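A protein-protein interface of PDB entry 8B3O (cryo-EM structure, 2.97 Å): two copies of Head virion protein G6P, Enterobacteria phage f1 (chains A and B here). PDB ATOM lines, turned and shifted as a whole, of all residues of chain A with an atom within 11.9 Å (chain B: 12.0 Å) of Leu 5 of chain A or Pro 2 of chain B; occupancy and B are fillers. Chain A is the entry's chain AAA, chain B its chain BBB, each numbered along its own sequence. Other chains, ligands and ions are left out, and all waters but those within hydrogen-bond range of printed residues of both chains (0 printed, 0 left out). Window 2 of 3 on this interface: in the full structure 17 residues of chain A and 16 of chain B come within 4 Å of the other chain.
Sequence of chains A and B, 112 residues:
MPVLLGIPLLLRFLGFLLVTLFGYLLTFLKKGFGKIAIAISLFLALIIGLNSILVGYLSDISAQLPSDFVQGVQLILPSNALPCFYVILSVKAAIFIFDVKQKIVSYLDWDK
Leu 5 of chain A touches Val 3 of chain B (O to CA, 3.8 Å). Gly 6 of chain A touches Val 3 of chain B (CA to CG1, 3.8 Å). CG2 of Ile 7 of chain B touches O of Gly 6 of chain A (3.96 Å). CD2 of Leu 9 of chain A touches CE of Met 1 of chain B (3.6 Å). Leu 10 of chain A touches Leu 11 of chain B (CD1 to CD2, 3.8 Å).
Val 3 of chain A touches none of the printed residues of chain B. No residue of chain B comes within 4 Å of Leu 4 of chain A. Printed residues of chain B within 4 Å of Leu 9 of chain A: Met 1 (3.6 Å). Of chain A, only Leu 5 comes within 4 Å of Pro 2 of chain B. No residue of chain A comes within 4 Å of Leu 4 of chain B. Of the printed residues of chain A, Ile 7 of chain B touches Gly 6. Pro 8 of chain B touches none of the printed residues of chain A. The nearest printed residue of chain B that does not touch Leu 9 of chain A is Leu 11 of chain B (4.3 Å).
O of Leu 5 of chain A lies close to O of Pro 2 of chain B, 3.1 Å away.
Hydrophobic or aromatic side chains of chain A that line the printed part of chain B: Leu 9 and Leu 10. Of the 11 printed residues of chain B, 5 touch a printed residue of chain A. Along chain B the printed residues that touch a printed residue of chain A span positions 1 to 11. Among the printed residues, 6 pairs touch across the chains.
Leu 5 of chain A touches Pro 2 of chain B, but with the chains exchanged Pro 2 of chain A does not touch Leu 5 of chain B (16.2 Å). Leu 5 of chain A touches Val 3 of chain B, but with the chains exchanged Val 3 of chain A does not touch Leu 5 of chain B (12.6 Å). Gly 6 of chain A touches Val 3 of chain B, but with the chains exchanged Val 3 of chain A does not touch Gly 6 of chain B (13.8 Å). Gly 6 of chain A touches Ile 7 of chain B, but with the chains exchanged Ile 7 of chain A does not touch Gly 6 of chain B (9.6 Å). Of the 6 pairs that touch across the chains among the printed residues, none has its exchanged pair printed and touching as well.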
ATOM      1  N   MET A   1      39.085  -8.541 -16.638  1.00  0.00           N
ATOM      2  CA  MET A   1      38.268  -7.674 -17.533  1.00  0.00           C
ATOM      3  C   MET A   1      36.820  -7.676 -17.040  1.00  0.00           C
ATOM      4  O   MET A   1      36.073  -8.615 -17.324  1.00  0.00           O
ATOM      5  CB  MET A   1      38.343  -8.156 -18.987  1.00  0.00           C
ATOM      6  CG  MET A   1      37.687  -7.206 -19.974  1.00  0.00           C
ATOM      7  SD  MET A   1      37.252  -8.008 -21.536  1.00  0.00           S
ATOM      8  CE  MET A   1      35.869  -9.014 -21.004  1.00  0.00           C
ATOM      9  N   PRO A   2      36.402  -6.625 -16.291  1.00  0.00           N
ATOM     10  CA  PRO A   2      35.096  -6.586 -15.626  1.00  0.00           C
ATOM     11  C   PRO A   2      33.925  -6.848 -16.569  1.00  0.00           C
ATOM     12  O   PRO A   2      33.907  -6.362 -17.698  1.00  0.00           O
ATOM     13  CB  PRO A   2      35.019  -5.158 -15.063  1.00  0.00           C
ATOM     14  CG  PRO A   2      36.465  -4.766 -14.862  1.00  0.00           C
ATOM     15  CD  PRO A   2      37.190  -5.408 -16.027  1.00  0.00           C
ATOM     16  N   VAL A   3      32.985  -7.668 -16.087  1.00  0.00           N
ATOM     17  CA  VAL A   3      31.780  -8.065 -16.799  1.00  0.00           C
ATOM     18  C   VAL A   3      30.633  -8.036 -15.788  1.00  0.00           C
ATOM     19  O   VAL A   3      30.886  -7.962 -14.589  1.00  0.00           O
ATOM     20  CB  VAL A   3      31.963  -9.459 -17.439  1.00  0.00           C
ATOM     21  CG1 VAL A   3      30.690  -9.984 -18.084  1.00  0.00           C
ATOM     22  CG2 VAL A   3      33.095  -9.494 -18.453  1.00  0.00           C
ATOM     23  N   LEU A   4      29.384  -8.090 -16.277  1.00  0.00           N
ATOM     24  CA  LEU A   4      28.192  -8.188 -15.444  1.00  0.00           C
ATOM     25  C   LEU A   4      28.131  -9.547 -14.744  1.00  0.00           C
ATOM     26  O   LEU A   4      29.014 -10.384 -14.922  1.00  0.00           O
ATOM     27  CB  LEU A   4      26.948  -7.931 -16.305  1.00  0.00           C
ATOM     28  CG  LEU A   4      26.740  -6.491 -16.776  1.00  0.00           C
ATOM     29  CD1 LEU A   4      25.659  -6.421 -17.844  1.00  0.00           C
ATOM     30  CD2 LEU A   4      26.399  -5.569 -15.613  1.00  0.00           C
ATOM     31  N   LEU A   5      27.064  -9.765 -13.963  1.00  0.00           N
ATOM     32  CA  LEU A   5      27.024 -10.827 -12.971  1.00  0.00           C
ATOM     33  C   LEU A   5      26.503 -12.153 -13.521  1.00  0.00           C
ATOM     34  O   LEU A   5      26.526 -13.150 -12.800  1.00  0.00           O
ATOM     35  CB  LEU A   5      26.199 -10.360 -11.769  1.00  0.00           C
ATOM     36  CG  LEU A   5      26.999  -9.651 -10.680  1.00  0.00           C
ATOM     37  CD1 LEU A   5      26.300  -9.773  -9.336  1.00  0.00           C
ATOM     38  CD2 LEU A   5      28.408 -10.215 -10.597  1.00  0.00           C
ATOM     39  N   GLY A   6      26.048 -12.167 -14.782  1.00  0.00           N
ATOM     40  CA  GLY A   6      25.412 -13.343 -15.354  1.00  0.00           C
ATOM     41  C   GLY A   6      26.006 -13.772 -16.694  1.00  0.00           C
ATOM     42  O   GLY A   6      25.658 -14.832 -17.209  1.00  0.00           O
ATOM     43  N   ILE A   7      26.897 -12.942 -17.249  1.00  0.00           N
ATOM     44  CA  ILE A   7      27.447 -13.190 -18.574  1.00  0.00           C
ATOM     45  C   ILE A   7      28.334 -14.441 -18.555  1.00  0.00           C
ATOM     46  O   ILE A   7      28.156 -15.294 -19.419  1.00  0.00           O
ATOM     47  CB  ILE A   7      28.116 -11.935 -19.186  1.00  0.00           C
ATOM     48  CG1 ILE A   7      27.212 -10.693 -19.160  1.00  0.00           C
ATOM     49  CG2 ILE A   7      28.685 -12.207 -20.577  1.00  0.00           C
ATOM     50  CD1 ILE A   7      26.030 -10.709 -20.120  1.00  0.00           C
ATOM     51  N   PRO A   8      29.276 -14.630 -17.591  1.00  0.00           N
ATOM     52  CA  PRO A   8      30.080 -15.859 -17.525  1.00  0.00           C
ATOM     53  C   PRO A   8      29.349 -17.204 -17.486  1.00  0.00           C
ATOM     54  O   PRO A   8      29.961 -18.230 -17.778  1.00  0.00           O
ATOM     55  CB  PRO A   8      30.906 -15.680 -16.240  1.00  0.00           C
ATOM     56  CG  PRO A   8      31.039 -14.186 -16.100  1.00  0.00           C
ATOM     57  CD  PRO A   8      29.700 -13.658 -16.566  1.00  0.00           C
ATOM     58  N   LEU A   9      28.054 -17.197 -17.125  1.00  0.00           N
ATOM     59  CA  LEU A   9      27.270 -18.423 -17.044  1.00  0.00           C
ATOM     60  C   LEU A   9      26.473 -18.653 -18.330  1.00  0.00           C
ATOM     61  O   LEU A   9      26.078 -19.784 -18.608  1.00  0.00           O
ATOM     62  CB  LEU A   9      26.382 -18.412 -15.789  1.00  0.00           C
ATOM     63  CG  LEU A   9      25.405 -19.582 -15.639  1.00  0.00           C
ATOM     64  CD1 LEU A   9      26.143 -20.887 -15.389  1.00  0.00           C
ATOM     65  CD2 LEU A   9      24.371 -19.322 -14.554  1.00  0.00           C
ATOM     66  N   LEU A  10      26.259 -17.586 -19.116  1.00  0.00           N
ATOM     67  CA  LEU A  10      25.662 -17.708 -20.436  1.00  0.00           C
ATOM     68  C   LEU A  10      26.693 -18.305 -21.393  1.00  0.00           C
ATOM     69  O   LEU A  10      26.325 -19.025 -22.318  1.00  0.00           O
ATOM     70  CB  LEU A  10      25.162 -16.334 -20.902  1.00  0.00           C
ATOM     71  CG  LEU A  10      24.586 -16.234 -22.318  1.00  0.00           C
ATOM     72  CD1 LEU A  10      23.343 -17.098 -22.484  1.00  0.00           C
ATOM     73  CD2 LEU A  10      24.275 -14.788 -22.674  1.00  0.00           C
ATOM     74  N   LEU A  11      27.979 -18.035 -21.124  1.00  0.00           N
ATOM     75  CA  LEU A  11      29.064 -18.436 -22.008  1.00  0.00           C
ATOM     76  C   LEU A  11      29.475 -19.885 -21.755  1.00  0.00           C
ATOM     77  O   LEU A  11      29.998 -20.537 -22.656  1.00  0.00           O
ATOM     78  CB  LEU A  11      30.250 -17.480 -21.844  1.00  0.00           C
ATOM     79  CG  LEU A  11      30.047 -16.045 -22.335  1.00  0.00           C
ATOM     80  CD1 LEU A  11      31.322 -15.234 -22.162  1.00  0.00           C
ATOM     81  CD2 LEU A  11      29.598 -16.010 -23.788  1.00  0.00           C
ATOM     82  N   ARG A  12      29.247 -20.371 -20.528  1.00  0.00           N
ATOM     83  CA  ARG A  12      29.540 -21.751 -20.167  1.00  0.00           C
ATOM     84  C   ARG A  12      28.417 -22.677 -20.639  1.00  0.00           C
ATOM     85  O   ARG A  12      28.676 -23.837 -20.953  1.00  0.00           O
ATOM     86  CB  ARG A  12      29.831 -21.881 -18.668  1.00  0.00           C
ATOM     87  CG  ARG A  12      31.259 -21.515 -18.288  1.00  0.00           C
ATOM     88  CD  ARG A  12      31.603 -21.838 -16.847  1.00  0.00           C
ATOM     89  NE  ARG A  12      31.495 -20.698 -15.943  1.00  0.00           N
ATOM     90  CZ  ARG A  12      30.555 -20.526 -15.015  1.00  0.00           C
ATOM     91  NH1 ARG A  12      29.590 -21.415 -14.857  1.00  0.00           N
ATOM     92  NH2 ARG A  12      30.579 -19.448 -14.251  1.00  0.00           N
ATOM     93  N   MET B   1      24.846 -18.698  -6.652  1.00  0.00           N
ATOM     94  CA  MET B   1      25.770 -17.877  -7.483  1.00  0.00           C
ATOM     95  C   MET B   1      24.982 -16.732  -8.120  1.00  0.00           C
ATOM     96  O   MET B   1      24.308 -16.935  -9.132  1.00  0.00           O
ATOM     97  CB  MET B   1      26.448 -18.728  -8.563  1.00  0.00           C
ATOM     98  CG  MET B   1      27.546 -17.990  -9.312  1.00  0.00           C
ATOM     99  SD  MET B   1      27.927 -18.738 -10.917  1.00  0.00           S
ATOM    100  CE  MET B   1      26.484 -18.234 -11.852  1.00  0.00           C
ATOM    101  N   PRO B   2      25.052 -15.508  -7.536  1.00  0.00           N
ATOM    102  CA  PRO B   2      24.222 -14.374  -7.953  1.00  0.00           C
ATOM    103  C   PRO B   2      24.312 -14.070  -9.445  1.00  0.00           C
ATOM    104  O   PRO B   2      25.390 -14.122 -10.033  1.00  0.00           O
ATOM    105  CB  PRO B   2      24.774 -13.198  -7.131  1.00  0.00           C
ATOM    106  CG  PRO B   2      25.358 -13.855  -5.902  1.00  0.00           C
ATOM    107  CD  PRO B   2      25.938 -15.157  -6.412  1.00  0.00           C
ATOM    108  N   VAL B   3      23.144 -13.803 -10.038  1.00  0.00           N
ATOM    109  CA  VAL B   3      22.979 -13.488 -11.449  1.00  0.00           C
ATOM    110  C   VAL B   3      21.969 -12.343 -11.539  1.00  0.00           C
ATOM    111  O   VAL B   3      21.294 -12.052 -10.555  1.00  0.00           O
ATOM    112  CB  VAL B   3      22.519 -14.738 -12.233  1.00  0.00           C
ATOM    113  CG1 VAL B   3      22.201 -14.439 -13.687  1.00  0.00           C
ATOM    114  CG2 VAL B   3      23.526 -15.874 -12.159  1.00  0.00           C
ATOM    115  N   LEU B   4      21.877 -11.700 -12.714  1.00  0.00           N
ATOM    116  CA  LEU B   4      20.889 -10.667 -12.997  1.00  0.00           C
ATOM    117  C   LEU B   4      19.480 -11.265 -13.047  1.00  0.00           C
ATOM    118  O   LEU B   4      19.305 -12.469 -12.867  1.00  0.00           O
ATOM    119  CB  LEU B   4      21.257  -9.957 -14.306  1.00  0.00           C
ATOM    120  CG  LEU B   4      22.487  -9.049 -14.257  1.00  0.00           C
ATOM    121  CD1 LEU B   4      22.922  -8.649 -15.658  1.00  0.00           C
ATOM    122  CD2 LEU B   4      22.231  -7.813 -13.406  1.00  0.00           C
ATOM    123  N   LEU B   5      18.485 -10.413 -13.326  1.00  0.00           N
ATOM    124  CA  LEU B   5      17.090 -10.733 -13.065  1.00  0.00           C
ATOM    125  C   LEU B   5      16.398 -11.431 -14.235  1.00  0.00           C
ATOM    126  O   LEU B   5      15.250 -11.848 -14.087  1.00  0.00           O
ATOM    127  CB  LEU B   5      16.346  -9.459 -12.659  1.00  0.00           C
ATOM    128  CG  LEU B   5      16.350  -9.165 -11.162  1.00  0.00           C
ATOM    129  CD1 LEU B   5      15.152  -8.310 -10.780  1.00  0.00           C
ATOM    130  CD2 LEU B   5      16.351 -10.459 -10.362  1.00  0.00           C
ATOM    131  N   GLY B   6      17.092 -11.568 -15.373  1.00  0.00           N
ATOM    132  CA  GLY B   6      16.482 -12.099 -16.582  1.00  0.00           C
ATOM    133  C   GLY B   6      17.269 -13.246 -17.214  1.00  0.00           C
ATOM    134  O   GLY B   6      16.785 -13.878 -18.151  1.00  0.00           O
ATOM    135  N   ILE B   7      18.477 -13.501 -16.701  1.00  0.00           N
ATOM    136  CA  ILE B   7      19.363 -14.495 -17.289  1.00  0.00           C
ATOM    137  C   ILE B   7      18.774 -15.900 -17.115  1.00  0.00           C
ATOM    138  O   ILE B   7      18.717 -16.634 -18.097  1.00  0.00           O
ATOM    139  CB  ILE B   7      20.826 -14.348 -16.805  1.00  0.00           C
ATOM    140  CG1 ILE B   7      21.373 -12.921 -16.963  1.00  0.00           C
ATOM    141  CG2 ILE B   7      21.746 -15.391 -17.435  1.00  0.00           C
ATOM    142  CD1 ILE B   7      21.647 -12.467 -18.390  1.00  0.00           C
ATOM    143  N   PRO B   8      18.292 -16.328 -15.916  1.00  0.00           N
ATOM    144  CA  PRO B   8      17.667 -17.648 -15.765  1.00  0.00           C
ATOM    145  C   PRO B   8      16.497 -18.013 -16.685  1.00  0.00           C
ATOM    146  O   PRO B   8      16.183 -19.195 -16.822  1.00  0.00           O
ATOM    147  CB  PRO B   8      17.206 -17.671 -14.299  1.00  0.00           C
ATOM    148  CG  PRO B   8      18.158 -16.729 -13.605  1.00  0.00           C
ATOM    149  CD  PRO B   8      18.394 -15.631 -14.620  1.00  0.00           C
ATOM    150  N   LEU B   9      15.864 -17.008 -17.310  1.00  0.00           N
ATOM    151  CA  LEU B   9      14.737 -17.244 -18.204  1.00  0.00           C
ATOM    152  C   LEU B   9      15.195 -17.301 -19.663  1.00  0.00           C
ATOM    153  O   LEU B   9      14.493 -17.865 -20.501  1.00  0.00           O
ATOM    154  CB  LEU B   9      13.636 -16.198 -17.968  1.00  0.00           C
ATOM    155  CG  LEU B   9      12.442 -16.241 -18.925  1.00  0.00           C
ATOM    156  CD1 LEU B   9      11.614 -17.498 -18.720  1.00  0.00           C
ATOM    157  CD2 LEU B   9      11.579 -14.993 -18.809  1.00  0.00           C
ATOM    158  N   LEU B  10      16.376 -16.735 -19.955  1.00  0.00           N
ATOM    159  CA  LEU B  10      16.992 -16.868 -21.266  1.00  0.00           C
ATOM    160  C   LEU B  10      17.547 -18.283 -21.413  1.00  0.00           C
ATOM    161  O   LEU B  10      17.564 -18.822 -22.516  1.00  0.00           O
ATOM    162  CB  LEU B  10      18.077 -15.794 -21.434  1.00  0.00           C
ATOM    163  CG  LEU B  10      18.917 -15.833 -22.715  1.00  0.00           C
ATOM    164  CD1 LEU B  10      18.064 -15.613 -23.956  1.00  0.00           C
ATOM    165  CD2 LEU B  10      20.039 -14.808 -22.655  1.00  0.00           C
ATOM    166  N   LEU B  11      17.945 -18.886 -20.283  1.00  0.00           N
ATOM    167  CA  LEU B  11      18.600 -20.186 -20.279  1.00  0.00           C
ATOM    168  C   LEU B  11      17.576 -21.318 -20.339  1.00  0.00           C
ATOM    169  O   LEU B  11      17.899 -22.407 -20.808  1.00  0.00           O
ATOM    170  CB  LEU B  11      19.499 -20.313 -19.043  1.00  0.00           C
ATOM    171  CG  LEU B  11      20.736 -19.414 -19.004  1.00  0.00           C
ATOM    172  CD1 LEU B  11      21.561 -19.692 -17.755  1.00  0.00           C
ATOM    173  CD2 LEU B  11      21.596 -19.588 -20.248  1.00  0.00           C
